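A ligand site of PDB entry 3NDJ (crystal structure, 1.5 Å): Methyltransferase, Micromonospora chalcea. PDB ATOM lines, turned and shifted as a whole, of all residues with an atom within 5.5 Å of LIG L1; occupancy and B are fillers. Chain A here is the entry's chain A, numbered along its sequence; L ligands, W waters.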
ATOM      1  N   ARG A  70     -13.378  34.851 -26.823  1.00  0.00           N
ATOM      2  CA  ARG A  70     -13.620  33.603 -27.560  1.00  0.00           C
ATOM      3  C   ARG A  70     -12.504  33.190 -28.507  1.00  0.00           C
ATOM      4  O   ARG A  70     -12.073  32.057 -28.558  1.00  0.00           O
ATOM      5  CB  ARG A  70     -15.003  33.613 -28.210  1.00  0.00           C
ATOM      6  CG  ARG A  70     -15.133  34.596 -29.381  1.00  0.00           C
ATOM      7  CD  ARG A  70     -16.545  34.521 -29.862  1.00  0.00           C
ATOM      8  NE  ARG A  70     -16.755  35.393 -31.019  1.00  0.00           N
ATOM      9  CZ  ARG A  70     -17.950  35.460 -31.588  1.00  0.00           C
ATOM     10  NH1 ARG A  70     -18.990  34.747 -31.204  1.00  0.00           N
ATOM     11  NH2 ARG A  70     -18.138  36.256 -32.615  1.00  0.00           N
ATOM     12  N   PHE A  74     -10.730  29.459 -29.029  1.00  0.00           N
ATOM     13  CA  PHE A  74     -11.336  28.594 -30.005  1.00  0.00           C
ATOM     14  C   PHE A  74     -10.881  29.212 -31.330  1.00  0.00           C
ATOM     15  O   PHE A  74     -11.168  30.358 -31.573  1.00  0.00           O
ATOM     16  CB  PHE A  74     -12.837  28.679 -29.840  1.00  0.00           C
ATOM     17  CG  PHE A  74     -13.292  28.273 -28.456  1.00  0.00           C
ATOM     18  CD1 PHE A  74     -12.972  27.015 -27.957  1.00  0.00           C
ATOM     19  CD2 PHE A  74     -14.054  29.138 -27.684  1.00  0.00           C
ATOM     20  CE1 PHE A  74     -13.383  26.658 -26.687  1.00  0.00           C
ATOM     21  CE2 PHE A  74     -14.512  28.793 -26.396  1.00  0.00           C
ATOM     22  CZ  PHE A  74     -14.161  27.514 -25.957  1.00  0.00           C
ATOM     23  N   TYR A  78      -7.291  24.682 -32.031  1.00  0.00           N
ATOM     24  CA  TYR A  78      -7.872  24.159 -30.778  1.00  0.00           C
ATOM     25  C   TYR A  78      -7.693  22.629 -30.708  1.00  0.00           C
ATOM     26  O   TYR A  78      -7.997  21.917 -31.670  1.00  0.00           O
ATOM     27  CB  TYR A  78      -9.380  24.463 -30.780  1.00  0.00           C
ATOM     28  CG  TYR A  78     -10.089  24.040 -29.505  1.00  0.00           C
ATOM     29  CD1 TYR A  78     -11.040  23.015 -29.533  1.00  0.00           C
ATOM     30  CD2 TYR A  78      -9.832  24.693 -28.322  1.00  0.00           C
ATOM     31  CE1 TYR A  78     -11.732  22.657 -28.391  1.00  0.00           C
ATOM     32  CE2 TYR A  78     -10.499  24.305 -27.148  1.00  0.00           C
ATOM     33  CZ  TYR A  78     -11.440  23.293 -27.219  1.00  0.00           C
ATOM     34  OH  TYR A  78     -12.137  22.951 -26.062  1.00  0.00           O
ATOM     35  N   TYR A  80      -8.762  19.889 -28.495  1.00  0.00           N
ATOM     36  CA  TYR A  80      -9.520  18.795 -27.887  1.00  0.00           C
ATOM     37  C   TYR A  80     -10.260  18.005 -28.956  1.00  0.00           C
ATOM     38  O   TYR A  80     -10.972  18.572 -29.813  1.00  0.00           O
ATOM     39  CB  TYR A  80     -10.611  19.349 -26.964  1.00  0.00           C
ATOM     40  CG  TYR A  80     -11.392  18.266 -26.290  1.00  0.00           C
ATOM     41  CD1 TYR A  80     -10.750  17.423 -25.398  1.00  0.00           C
ATOM     42  CD2 TYR A  80     -12.760  18.120 -26.515  1.00  0.00           C
ATOM     43  CE1 TYR A  80     -11.475  16.399 -24.726  1.00  0.00           C
ATOM     44  CE2 TYR A  80     -13.459  17.119 -25.872  1.00  0.00           C
ATOM     45  CZ  TYR A  80     -12.814  16.290 -24.980  1.00  0.00           C
ATOM     46  OH  TYR A  80     -13.513  15.325 -24.328  1.00  0.00           O
ATOM     47  N   SER A  82     -13.093  15.335 -29.327  1.00  0.00           N
ATOM     48  CA  SER A  82     -14.146  14.589 -28.632  1.00  0.00           C
ATOM     49  C   SER A  82     -14.034  13.076 -28.804  1.00  0.00           C
ATOM     50  O   SER A  82     -14.321  12.350 -27.838  1.00  0.00           O
ATOM     51  CB  SER A  82     -15.532  15.062 -29.075  1.00  0.00           C
ATOM     52  OG  SER A  82     -15.609  16.446 -28.826  1.00  0.00           O
ATOM     53  N   PHE A  92     -22.711   9.775 -27.311  1.00  0.00           N
ATOM     54  CA  PHE A  92     -23.320  10.684 -28.273  1.00  0.00           C
ATOM     55  C   PHE A  92     -24.065   9.978 -29.415  1.00  0.00           C
ATOM     56  O   PHE A  92     -25.074  10.491 -29.934  1.00  0.00           O
ATOM     57  CB  PHE A  92     -22.270  11.647 -28.830  1.00  0.00           C
ATOM     58  CG  PHE A  92     -21.855  12.687 -27.839  1.00  0.00           C
ATOM     59  CD1 PHE A  92     -22.797  13.594 -27.364  1.00  0.00           C
ATOM     60  CD2 PHE A  92     -20.526  12.771 -27.380  1.00  0.00           C
ATOM     61  CE1 PHE A  92     -22.419  14.559 -26.459  1.00  0.00           C
ATOM     62  CE2 PHE A  92     -20.144  13.749 -26.474  1.00  0.00           C
ATOM     63  CZ  PHE A  92     -21.094  14.629 -26.000  1.00  0.00           C
ATOM     64  N   GLU A 113     -26.221  21.320 -34.451  1.00  0.00           N
ATOM     65  CA  GLU A 113     -25.419  21.174 -33.254  1.00  0.00           C
ATOM     66  C   GLU A 113     -24.460  22.347 -33.113  1.00  0.00           C
ATOM     67  O   GLU A 113     -23.740  22.699 -34.037  1.00  0.00           O
ATOM     68  CB  GLU A 113     -24.621  19.853 -33.284  1.00  0.00           C
ATOM     69  CG  GLU A 113     -23.886  19.648 -31.957  1.00  0.00           C
ATOM     70  CD  GLU A 113     -23.082  18.381 -31.843  1.00  0.00           C
ATOM     71  OE1 GLU A 113     -22.670  17.997 -30.706  1.00  0.00           O
ATOM     72  OE2 GLU A 113     -22.846  17.730 -32.871  1.00  0.00           O
ATOM     73  N   ILE A 114     -24.431  22.921 -31.910  1.00  0.00           N
ATOM     74  CA  ILE A 114     -23.515  23.960 -31.495  1.00  0.00           C
ATOM     75  C   ILE A 114     -22.307  23.266 -30.880  1.00  0.00           C
ATOM     76  O   ILE A 114     -22.411  22.577 -29.840  1.00  0.00           O
ATOM     77  CB  ILE A 114     -24.190  24.912 -30.470  1.00  0.00           C
ATOM     78  CG1 ILE A 114     -25.433  25.549 -31.079  1.00  0.00           C
ATOM     79  CG2 ILE A 114     -23.243  26.038 -30.089  1.00  0.00           C
ATOM     80  CD1 ILE A 114     -26.318  26.354 -30.102  1.00  0.00           C
ATOM     81  N   GLY A 115     -21.140  23.474 -31.474  1.00  0.00           N
ATOM     82  CA  GLY A 115     -19.895  22.883 -30.991  1.00  0.00           C
ATOM     83  C   GLY A 115     -19.713  21.439 -31.400  1.00  0.00           C
ATOM     84  O   GLY A 115     -19.464  20.571 -30.523  1.00  0.00           O
ATOM     85  N   CYS A 116     -19.866  21.091 -32.683  1.00  0.00           N
ATOM     86  CA  CYS A 116     -19.812  19.674 -33.088  1.00  0.00           C
ATOM     87  C   CYS A 116     -18.460  19.020 -32.971  1.00  0.00           C
ATOM     88  O   CYS A 116     -18.393  17.774 -33.035  1.00  0.00           O
ATOM     89  CB  CYS A 116     -20.413  19.390 -34.477  1.00  0.00           C
ATOM     90  SG  CYS A 116     -19.512  20.239 -35.795  1.00  0.00           S
ATOM     91  N   ASN A 117     -17.404  19.816 -32.827  1.00  0.00           N
ATOM     92  CA  ASN A 117     -16.027  19.312 -32.768  1.00  0.00           C
ATOM     93  C   ASN A 117     -15.779  18.361 -33.918  1.00  0.00           C
ATOM     94  O   ASN A 117     -16.157  18.670 -35.039  1.00  0.00           O
ATOM     95  CB  ASN A 117     -15.827  18.714 -31.371  1.00  0.00           C
ATOM     96  CG  ASN A 117     -14.358  18.491 -31.000  1.00  0.00           C
ATOM     97  OD1 ASN A 117     -13.828  17.395 -31.212  1.00  0.00           O
ATOM     98  ND2 ASN A 117     -13.689  19.482 -30.406  1.00  0.00           N
ATOM     99  N   ILE A 120     -18.412  13.827 -33.442  1.00  0.00           N
ATOM    100  CA  ILE A 120     -18.767  12.711 -32.546  1.00  0.00           C
ATOM    101  C   ILE A 120     -20.286  12.399 -32.448  1.00  0.00           C
ATOM    102  O   ILE A 120     -20.723  11.232 -32.336  1.00  0.00           O
ATOM    103  CB  ILE A 120     -18.196  12.987 -31.127  1.00  0.00           C
ATOM    104  CG1 ILE A 120     -18.316  11.749 -30.254  1.00  0.00           C
ATOM    105  CG2 ILE A 120     -18.800  14.244 -30.454  1.00  0.00           C
ATOM    106  CD1 ILE A 120     -17.458  11.836 -29.007  1.00  0.00           C
ATOM    107  N   PHE A 135     -22.127  23.801 -36.078  1.00  0.00           N
ATOM    108  CA  PHE A 135     -21.293  24.999 -35.891  1.00  0.00           C
ATOM    109  C   PHE A 135     -20.030  24.580 -35.138  1.00  0.00           C
ATOM    110  O   PHE A 135     -20.084  24.058 -34.031  1.00  0.00           O
ATOM    111  CB  PHE A 135     -21.975  26.121 -35.113  1.00  0.00           C
ATOM    112  CG  PHE A 135     -23.058  26.851 -35.842  1.00  0.00           C
ATOM    113  CD1 PHE A 135     -22.862  28.171 -36.206  1.00  0.00           C
ATOM    114  CD2 PHE A 135     -24.296  26.268 -36.105  1.00  0.00           C
ATOM    115  CE1 PHE A 135     -23.860  28.890 -36.871  1.00  0.00           C
ATOM    116  CE2 PHE A 135     -25.306  26.984 -36.777  1.00  0.00           C
ATOM    117  CZ  PHE A 135     -25.059  28.305 -37.158  1.00  0.00           C
ATOM    118  N   GLU A 136     -18.881  24.836 -35.729  1.00  0.00           N
ATOM    119  CA  GLU A 136     -17.611  24.528 -35.107  1.00  0.00           C
ATOM    120  C   GLU A 136     -16.611  25.611 -35.534  1.00  0.00           C
ATOM    121  O   GLU A 136     -16.054  25.484 -36.625  1.00  0.00           O
ATOM    122  CB  GLU A 136     -17.149  23.142 -35.576  1.00  0.00           C
ATOM    123  CG  GLU A 136     -15.912  22.590 -34.821  1.00  0.00           C
ATOM    124  CD  GLU A 136     -15.850  23.195 -33.448  1.00  0.00           C
ATOM    125  OE1 GLU A 136     -16.491  22.502 -32.603  1.00  0.00           O
ATOM    126  OE2 GLU A 136     -15.266  24.299 -33.233  1.00  0.00           O
ATOM    127  N   PRO A 137     -16.411  26.633 -34.691  1.00  0.00           N
ATOM    128  CA  PRO A 137     -15.544  27.771 -35.028  1.00  0.00           C
ATOM    129  C   PRO A 137     -14.074  27.397 -35.006  1.00  0.00           C
ATOM    130  O   PRO A 137     -13.232  28.221 -35.384  1.00  0.00           O
ATOM    131  CB  PRO A 137     -15.812  28.772 -33.889  1.00  0.00           C
ATOM    132  CG  PRO A 137     -16.246  27.897 -32.727  1.00  0.00           C
ATOM    133  CD  PRO A 137     -17.067  26.825 -33.391  1.00  0.00           C
ATOM    134  N   SER A 138     -13.737  26.201 -34.512  1.00  0.00           N
ATOM    135  CA  SER A 138     -12.344  25.758 -34.445  1.00  0.00           C
ATOM    136  C   SER A 138     -12.150  24.905 -35.693  1.00  0.00           C
ATOM    137  O   SER A 138     -12.615  23.780 -35.790  1.00  0.00           O
ATOM    138  CB  SER A 138     -12.037  24.937 -33.172  1.00  0.00           C
ATOM    139  OG  SER A 138     -12.141  25.776 -32.039  1.00  0.00           O
ATOM    140  N   VAL A 141     -10.615  20.967 -35.937  1.00  0.00           N
ATOM    141  CA  VAL A 141     -11.530  19.850 -35.617  1.00  0.00           C
ATOM    142  C   VAL A 141     -12.757  19.876 -36.554  1.00  0.00           C
ATOM    143  O   VAL A 141     -13.334  18.832 -36.880  1.00  0.00           O
ATOM    144  CB  VAL A 141     -11.951  19.849 -34.124  1.00  0.00           C
ATOM    145  CG1 VAL A 141     -10.732  19.621 -33.266  1.00  0.00           C
ATOM    146  CG2 VAL A 141     -12.664  21.180 -33.745  1.00  0.00           C
ATOM    147  N   ASP A 155     -17.974  28.735 -37.741  1.00  0.00           N
ATOM    148  CA  ASP A 155     -18.484  30.009 -37.252  1.00  0.00           C
ATOM    149  C   ASP A 155     -18.913  29.726 -35.821  1.00  0.00           C
ATOM    150  O   ASP A 155     -19.248  28.591 -35.467  1.00  0.00           O
ATOM    151  CB  ASP A 155     -19.780  30.408 -37.974  1.00  0.00           C
ATOM    152  CG  ASP A 155     -19.538  31.276 -39.165  1.00  0.00           C
ATOM    153  OD1 ASP A 155     -20.021  30.865 -40.242  1.00  0.00           O
ATOM    154  OD2 ASP A 155     -18.851  32.317 -38.996  1.00  0.00           O
ATOM    155  N   PHE A 156     -18.899  30.755 -34.992  1.00  0.00           N
ATOM    156  CA  PHE A 156     -19.545  30.665 -33.664  1.00  0.00           C
ATOM    157  C   PHE A 156     -21.043  30.819 -33.922  1.00  0.00           C
ATOM    158  O   PHE A 156     -21.520  31.637 -34.749  1.00  0.00           O
ATOM    159  CB  PHE A 156     -19.115  31.904 -32.870  1.00  0.00           C
ATOM    160  CG  PHE A 156     -17.645  31.887 -32.518  1.00  0.00           C
ATOM    161  CD1 PHE A 156     -17.185  31.032 -31.528  1.00  0.00           C
ATOM    162  CD2 PHE A 156     -16.739  32.665 -33.209  1.00  0.00           C
ATOM    163  CE1 PHE A 156     -15.832  30.981 -31.219  1.00  0.00           C
ATOM    164  CE2 PHE A 156     -15.383  32.629 -32.913  1.00  0.00           C
ATOM    165  CZ  PHE A 156     -14.918  31.787 -31.909  1.00  0.00           C
ATOM    166  N   PHE A 157     -21.826  30.028 -33.206  1.00  0.00           N
ATOM    167  CA  PHE A 157     -23.249  30.233 -33.119  1.00  0.00           C
ATOM    168  C   PHE A 157     -23.483  31.436 -32.214  1.00  0.00           C
ATOM    169  O   PHE A 157     -22.925  31.534 -31.115  1.00  0.00           O
ATOM    170  CB  PHE A 157     -23.880  28.979 -32.465  1.00  0.00           C
ATOM    171  CG  PHE A 157     -25.382  29.011 -32.515  1.00  0.00           C
ATOM    172  CD1 PHE A 157     -26.083  29.843 -31.664  1.00  0.00           C
ATOM    173  CD2 PHE A 157     -26.110  28.267 -33.476  1.00  0.00           C
ATOM    174  CE1 PHE A 157     -27.490  29.923 -31.733  1.00  0.00           C
ATOM    175  CE2 PHE A 157     -27.522  28.334 -33.560  1.00  0.00           C
ATOM    176  CZ  PHE A 157     -28.206  29.146 -32.683  1.00  0.00           C
ATOM    177  N   GLU A 158     -24.345  32.334 -32.711  1.00  0.00           N
ATOM    178  CA  GLU A 158     -24.799  33.521 -32.010  1.00  0.00           C
ATOM    179  C   GLU A 158     -25.992  34.026 -32.835  1.00  0.00           C
ATOM    180  O   GLU A 158     -26.363  33.376 -33.789  1.00  0.00           O
ATOM    181  CB  GLU A 158     -23.702  34.596 -32.019  1.00  0.00           C
ATOM    182  CG  GLU A 158     -23.177  34.954 -33.411  1.00  0.00           C
ATOM    183  CD  GLU A 158     -22.075  35.977 -33.430  1.00  0.00           C
ATOM    184  OE1 GLU A 158     -22.299  37.181 -33.732  1.00  0.00           O
ATOM    185  OE2 GLU A 158     -20.921  35.614 -33.135  1.00  0.00           O
ATOM    186  N   ALA A 178     -23.489  20.130 -26.476  1.00  0.00           N
ATOM    187  CA  ALA A 178     -22.902  19.391 -25.341  1.00  0.00           C
ATOM    188  C   ALA A 178     -21.536  19.994 -24.974  1.00  0.00           C
ATOM    189  O   ALA A 178     -20.717  20.165 -25.878  1.00  0.00           O
ATOM    190  CB  ALA A 178     -22.821  17.882 -25.632  1.00  0.00           C
ATOM    191  N   ASN A 179     -21.284  20.242 -23.674  1.00  0.00           N
ATOM    192  CA  ASN A 179     -20.002  20.875 -23.292  1.00  0.00           C
ATOM    193  C   ASN A 179     -19.622  22.072 -24.158  1.00  0.00           C
ATOM    194  O   ASN A 179     -18.443  22.239 -24.485  1.00  0.00           O
ATOM    195  CB  ASN A 179     -18.919  19.808 -23.338  1.00  0.00           C
ATOM    196  CG  ASN A 179     -19.399  18.583 -22.580  1.00  0.00           C
ATOM    197  OD1 ASN A 179     -19.620  18.683 -21.366  1.00  0.00           O
ATOM    198  ND2 ASN A 179     -19.590  17.475 -23.293  1.00  0.00           N
ATOM    199  N   THR A 180     -20.619  22.876 -24.471  1.00  0.00           N
ATOM    200  CA  THR A 180     -20.439  24.060 -25.316  1.00  0.00           C
ATOM    201  C   THR A 180     -21.189  25.272 -24.762  1.00  0.00           C
ATOM    202  O   THR A 180     -20.679  26.386 -24.712  1.00  0.00           O
ATOM    203  CB  THR A 180     -20.863  23.804 -26.787  1.00  0.00           C
ATOM    204  OG1 THR A 180     -20.057  22.752 -27.309  1.00  0.00           O
ATOM    205  CG2 THR A 180     -20.495  24.988 -27.624  1.00  0.00           C
ATOM    206  N   HIS A 183     -19.674  27.297 -22.152  1.00  0.00           N
ATOM    207  CA  HIS A 183     -18.441  27.937 -22.603  1.00  0.00           C
ATOM    208  C   HIS A 183     -18.700  29.355 -23.127  1.00  0.00           C
ATOM    209  O   HIS A 183     -17.706  30.009 -23.375  1.00  0.00           O
ATOM    210  CB  HIS A 183     -17.820  27.135 -23.745  1.00  0.00           C
ATOM    211  CG  HIS A 183     -17.329  25.768 -23.342  1.00  0.00           C
ATOM    212  ND1 HIS A 183     -18.057  24.916 -22.534  1.00  0.00           N
ATOM    213  CD2 HIS A 183     -16.182  25.101 -23.630  1.00  0.00           C
ATOM    214  CE1 HIS A 183     -17.380  23.805 -22.325  1.00  0.00           C
ATOM    215  NE2 HIS A 183     -16.243  23.884 -22.987  1.00  0.00           N
ATOM    216  N   ILE A 184     -19.943  29.775 -23.306  1.00  0.00           N
ATOM    217  CA  ILE A 184     -20.233  30.966 -24.087  1.00  0.00           C
ATOM    218  C   ILE A 184     -20.827  32.024 -23.169  1.00  0.00           C
ATOM    219  O   ILE A 184     -21.993  32.005 -22.785  1.00  0.00           O
ATOM    220  CB  ILE A 184     -21.256  30.613 -25.206  1.00  0.00           C
ATOM    221  CG1 ILE A 184     -20.624  29.606 -26.195  1.00  0.00           C
ATOM    222  CG2 ILE A 184     -21.795  31.863 -25.930  1.00  0.00           C
ATOM    223  CD1 ILE A 184     -21.617  28.962 -27.160  1.00  0.00           C
ATOM    224  N   TYR A 186     -21.688  34.950 -23.896  1.00  0.00           N
ATOM    225  CA  TYR A 186     -22.760  35.639 -24.607  1.00  0.00           C
ATOM    226  C   TYR A 186     -24.008  34.780 -24.854  1.00  0.00           C
ATOM    227  O   TYR A 186     -24.524  34.650 -25.978  1.00  0.00           O
ATOM    228  CB  TYR A 186     -22.220  36.255 -25.903  1.00  0.00           C
ATOM    229  CG  TYR A 186     -21.399  35.288 -26.755  1.00  0.00           C
ATOM    230  CD1 TYR A 186     -20.022  35.132 -26.566  1.00  0.00           C
ATOM    231  CD2 TYR A 186     -22.014  34.514 -27.754  1.00  0.00           C
ATOM    232  CE1 TYR A 186     -19.300  34.241 -27.357  1.00  0.00           C
ATOM    233  CE2 TYR A 186     -21.302  33.618 -28.524  1.00  0.00           C
ATOM    234  CZ  TYR A 186     -19.951  33.476 -28.311  1.00  0.00           C
ATOM    235  OH  TYR A 186     -19.245  32.596 -29.080  1.00  0.00           O
ATOM    236  N   VAL A 190     -26.791  33.689 -27.957  1.00  0.00           N
ATOM    237  CA  VAL A 190     -27.112  32.291 -28.312  1.00  0.00           C
ATOM    238  C   VAL A 190     -28.625  32.089 -28.246  1.00  0.00           C
ATOM    239  O   VAL A 190     -29.187  31.578 -29.208  1.00  0.00           O
ATOM    240  CB  VAL A 190     -26.328  31.258 -27.476  1.00  0.00           C
ATOM    241  CG1 VAL A 190     -26.711  29.818 -27.814  1.00  0.00           C
ATOM    242  CG2 VAL A 190     -24.820  31.436 -27.643  1.00  0.00           C
ATOM    243  N   HIS A 256     -18.175  13.339 -17.845  1.00  0.00           N
ATOM    244  CA  HIS A 256     -17.473  14.569 -17.490  1.00  0.00           C
ATOM    245  C   HIS A 256     -17.592  15.015 -16.041  1.00  0.00           C
ATOM    246  O   HIS A 256     -17.698  16.200 -15.756  1.00  0.00           O
ATOM    247  CB  HIS A 256     -17.824  15.700 -18.433  1.00  0.00           C
ATOM    248  CG  HIS A 256     -17.270  15.457 -19.791  1.00  0.00           C
ATOM    249  ND1 HIS A 256     -15.909  15.338 -20.019  1.00  0.00           N
ATOM    250  CD2 HIS A 256     -17.870  15.271 -20.991  1.00  0.00           C
ATOM    251  CE1 HIS A 256     -15.711  15.093 -21.301  1.00  0.00           C
ATOM    252  NE2 HIS A 256     -16.875  15.057 -21.912  1.00  0.00           N
HETATM  253  N1  LIG L   1     -19.785  18.600 -28.165  1.00  0.00           N
HETATM  254  C1  LIG L   1     -18.358  18.214 -28.119  1.00  0.00           C
HETATM  255  C2  LIG L   1     -17.514  19.478 -28.270  1.00  0.00           C
HETATM  256  C3  LIG L   1     -16.754  19.810 -26.991  1.00  0.00           C
HETATM  257  S1  LIG L   1     -15.493  20.989 -27.340  1.00  0.00           S
HETATM  258  C4  LIG L   1     -18.320  17.400 -26.861  1.00  0.00           C
HETATM  259  O1  LIG L   1     -19.281  17.484 -26.098  1.00  0.00           O
HETATM  260  O2  LIG L   1     -17.320  16.710 -26.734  1.00  0.00           O
HETATM  261  C5  LIG L   1     -16.369  22.528 -27.330  1.00  0.00           C
HETATM  262  C6  LIG L   1     -16.437  23.084 -28.746  1.00  0.00           C
HETATM  263  O3  LIG L   1     -17.258  24.255 -28.644  1.00  0.00           O
HETATM  264  C7  LIG L   1     -15.086  23.557 -29.349  1.00  0.00           C
HETATM  265  O4  LIG L   1     -14.833  22.737 -30.493  1.00  0.00           O
HETATM  266  C8  LIG L   1     -15.309  25.011 -29.697  1.00  0.00           C
HETATM  267  O5  LIG L   1     -14.696  25.415 -30.937  1.00  0.00           O
HETATM  268  C9  LIG L   1     -16.835  25.044 -29.781  1.00  0.00           C
HETATM  269  N2  LIG L   1     -17.414  26.396 -29.603  1.00  0.00           N
HETATM  270  C10 LIG L   1     -17.062  27.423 -28.827  1.00  0.00           C
HETATM  271  N3  LIG L   1     -17.845  28.514 -28.874  1.00  0.00           N
HETATM  272  C11 LIG L   1     -18.781  28.147 -29.801  1.00  0.00           C
HETATM  273  C12 LIG L   1     -20.001  28.748 -30.385  1.00  0.00           C
HETATM  274  N4  LIG L   1     -20.302  30.036 -30.032  1.00  0.00           N
HETATM  275  N5  LIG L   1     -20.645  27.994 -31.296  1.00  0.00           N
HETATM  276  C13 LIG L   1     -20.395  26.714 -31.666  1.00  0.00           C
HETATM  277  N6  LIG L   1     -19.298  26.120 -31.201  1.00  0.00           N
HETATM  278  C14 LIG L   1     -18.540  26.747 -30.255  1.00  0.00           C
HETATM  279  P1  LG2 L   2     -11.416  15.250 -21.115  1.00  0.00           P
HETATM  280  C1  LG2 L   2     -12.125  19.378 -22.832  1.00  0.00           C
HETATM  281  O1  LG2 L   2     -11.913  19.327 -21.431  1.00  0.00           O
HETATM  282  C2  LG2 L   2     -12.318  20.876 -23.201  1.00  0.00           C
HETATM  283  P2  LG2 L   2     -10.926  18.181 -20.891  1.00  0.00           P
HETATM  284  C3  LG2 L   2     -13.788  21.320 -23.078  1.00  0.00           C
HETATM  285  N1  LG2 L   2     -13.805  22.680 -22.551  1.00  0.00           N
HETATM  286  C4  LG2 L   2     -14.590  20.398 -22.182  1.00  0.00           C
HETATM  287  O2  LG2 L   2     -15.439  20.765 -21.364  1.00  0.00           O
HETATM  288  C5  LG2 L   2     -14.446  18.912 -22.292  1.00  0.00           C
HETATM  289  O3  LG2 L   2     -13.326  18.722 -23.165  1.00  0.00           O
HETATM  290  C6  LG2 L   2     -15.652  18.197 -22.862  1.00  0.00           C
HETATM  291  C7  LG2 L   2      -6.833  12.053 -22.743  1.00  0.00           C
HETATM  292  N2  LG2 L   2      -7.239  10.630 -22.688  1.00  0.00           N
HETATM  293  O4  LG2 L   2     -12.285  14.530 -22.093  1.00  0.00           O
HETATM  294  C8  LG2 L   2      -7.440  12.741 -23.950  1.00  0.00           C
HETATM  295  C9  LG2 L   2      -6.305   9.669 -22.725  1.00  0.00           C
HETATM  296  O5  LG2 L   2      -5.089   9.922 -22.782  1.00  0.00           O
HETATM  297  O6  LG2 L   2     -11.523  14.843 -19.664  1.00  0.00           O
HETATM  298  C10 LG2 L   2      -7.758  14.162 -23.489  1.00  0.00           C
HETATM  299  O7  LG2 L   2      -6.680  15.095 -23.752  1.00  0.00           O
HETATM  300  N3  LG2 L   2      -6.677   8.368 -22.653  1.00  0.00           N
HETATM  301  C11 LG2 L   2     -14.490  21.401 -24.470  1.00  0.00           C
HETATM  302  O8  LG2 L   2      -9.588  18.308 -21.552  1.00  0.00           O
HETATM  303  C12 LG2 L   2      -7.931  14.035 -21.978  1.00  0.00           C
HETATM  304  O9  LG2 L   2      -7.254  12.840 -21.638  1.00  0.00           O
HETATM  305  C13 LG2 L   2      -7.969   8.042 -22.658  1.00  0.00           C
HETATM  306  O10 LG2 L   2      -8.264   6.721 -22.592  1.00  0.00           O
HETATM  307  O11 LG2 L   2     -10.868  18.345 -19.411  1.00  0.00           O
HETATM  308  C14 LG2 L   2      -9.324  13.845 -21.408  1.00  0.00           C
HETATM  309  O12 LG2 L   2      -9.870  15.145 -21.526  1.00  0.00           O
HETATM  310  C15 LG2 L   2      -8.970   8.985 -22.610  1.00  0.00           C
HETATM  311  C16 LG2 L   2     -10.436   8.681 -22.537  1.00  0.00           C
HETATM  312  C17 LG2 L   2      -8.542  10.312 -22.599  1.00  0.00           C
HETATM  313  O13 LG2 L   2     -11.642  16.828 -21.392  1.00  0.00           O
HETATM  314  O   HOH W   1     -21.182  16.450 -29.264  1.00  0.00           O
HETATM  315  O   HOH W   2     -17.337  31.144 -27.998  1.00  0.00           O
HETATM  316  O   HOH W   3     -22.264  20.097 -29.018  1.00  0.00           O
HETATM  317  O   HOH W   4     -16.913  14.904 -24.749  1.00  0.00           O
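The side-chain hydroxyl (OG) of Ser 138 is in hydrogen-bond range of an oxygen (O5) of LIG L1, 2.8 Å away.
An oxygen (O2) of LIG L1 sits at hydrogen-bond distance from the side-chain hydroxyl (OG) of Ser 82 (2.7 Å).
N of Phe 157 lies within hydrogen-bond range of N5 of LIG L1 (3.0 Å).
The backbone carbonyl oxygen (O) of Ala 178 sits at hydrogen-bond distance from a nitrogen (N1) of LIG L1.
The side-chain hydroxyl (OG1) of Thr 180 is in hydrogen-bond range of an oxygen (O3) of LIG L1, at 3.4 Å.
The side-chain hydroxyl (OH) of Tyr 186 sits at hydrogen-bond distance from a nitrogen (N4) of LIG L1 (2.9 Å).
The side-chain carboxylate (OE2) of Glu 136 sits at hydrogen-bond distance from an oxygen (O5) of LIG L1 (2.6 Å).
A nitrogen (N1) of LIG L1 is in salt-bridge range of the side-chain carboxylate of Glu 113 (3.9 Å).
ND2 of Asn 117 is in hydrogen-bond range of O4 of LIG L1 (3.5 Å).
O of Gly 115 sits at hydrogen-bond distance from N1 of LIG L1 (3.1 Å).
OH of Tyr 80 lies within hydrogen-bond range of O4 of LG2 L2, 2.7 Å away.
The backbone carbonyl oxygen (O) of Phe 157 is in hydrogen-bond range of a nitrogen (N4) of LIG L1.
NE2 of His 183 sits at hydrogen-bond distance from N1 of LG2 L2, 2.8 Å away.
N6 of LIG L1 sits at hydrogen-bond distance from N of Gly 115 (3.2 Å).
ND2 of Asn 179 lies within hydrogen-bond range of O1 of LIG L1 (2.8 Å).
OE2 of Glu 136 lies within hydrogen-bond range of N of Ser 138 (2.8 Å).
The side-chain hydroxyl (OH) of Tyr 186 lies within hydrogen-bond range of the guanidinium group (NH1) of Arg 70 (3.0 Å).
The side-chain hydroxyl (OG1) of Thr 180 is in hydrogen-bond range of the backbone carbonyl oxygen (O) of Ile 114 (3.5 Å).
N of Gly 115 sits at hydrogen-bond distance from O of Phe 135 (2.8 Å).
The side-chain amide oxygen (OD1) of Asn 117 lies within hydrogen-bond range of the backbone NH (N) of Ser 82 (2.9 Å).
The backbone carbonyl oxygen of Tyr 80 lies within hydrogen-bond range of the side-chain amide nitrogen of Asn 117 (2.9 Å).
The side-chain carboxylate (OE1) of Glu 136 sits at hydrogen-bond distance from the backbone NH (N) of Asn 117, at 2.8 Å.
The backbone NH of Phe 135 sits at hydrogen-bond distance from the backbone carbonyl oxygen of Glu 113.
Phe 74 touches LIG L1.
Tyr 78 touches LIG L1 (CE1 to C7, 3.6 Å).
CE2 of Tyr 80 touches O2 of LIG L1, 3.98 Å away.
Phe 92 touches LIG L1 (CZ to O1, 3.4 Å).
Ile 114 touches LIG L1.
O of Phe 135 touches C13 of LIG L1, at 3.6 Å.
CD of Pro 137 touches N6 of LIG L1, 3.2 Å away.
Phe 156 touches LIG L1.
Ile 184 touches LIG L1 (CD1 to N4, 3.3 Å).
20 residues have an atom within 4 Å of LIG L1: Phe 74, Tyr 78, Tyr 80, Ser 82, Phe 92, Glu 113, Ile 114, Gly 115, Asn 117, Phe 135, Glu 136, Pro 137, Ser 138, Phe 156, Phe 157, Ala 178, Asn 179, Thr 180, Ile 184 and Tyr 186.
The nearest printed residue that does not touch LIG L1 is Val 141 (4.2 Å).
Water W4 lies within hydrogen-bond range of an oxygen (O2) of LIG L1 (2.7 Å), a ring nitrogen (NE2) of His 256 (2.8 Å) and the side-chain hydroxyl of Tyr 80 (3.5 Å).
Water W1 bridges the side-chain carboxylate of Glu 113 (2.6 Å) and a nitrogen (N1) of LIG L1 (2.8 Å).
Water W2 lies within hydrogen-bond range of the side-chain hydroxyl (OH) of Tyr 186 and a nitrogen (N3) of LIG L1.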
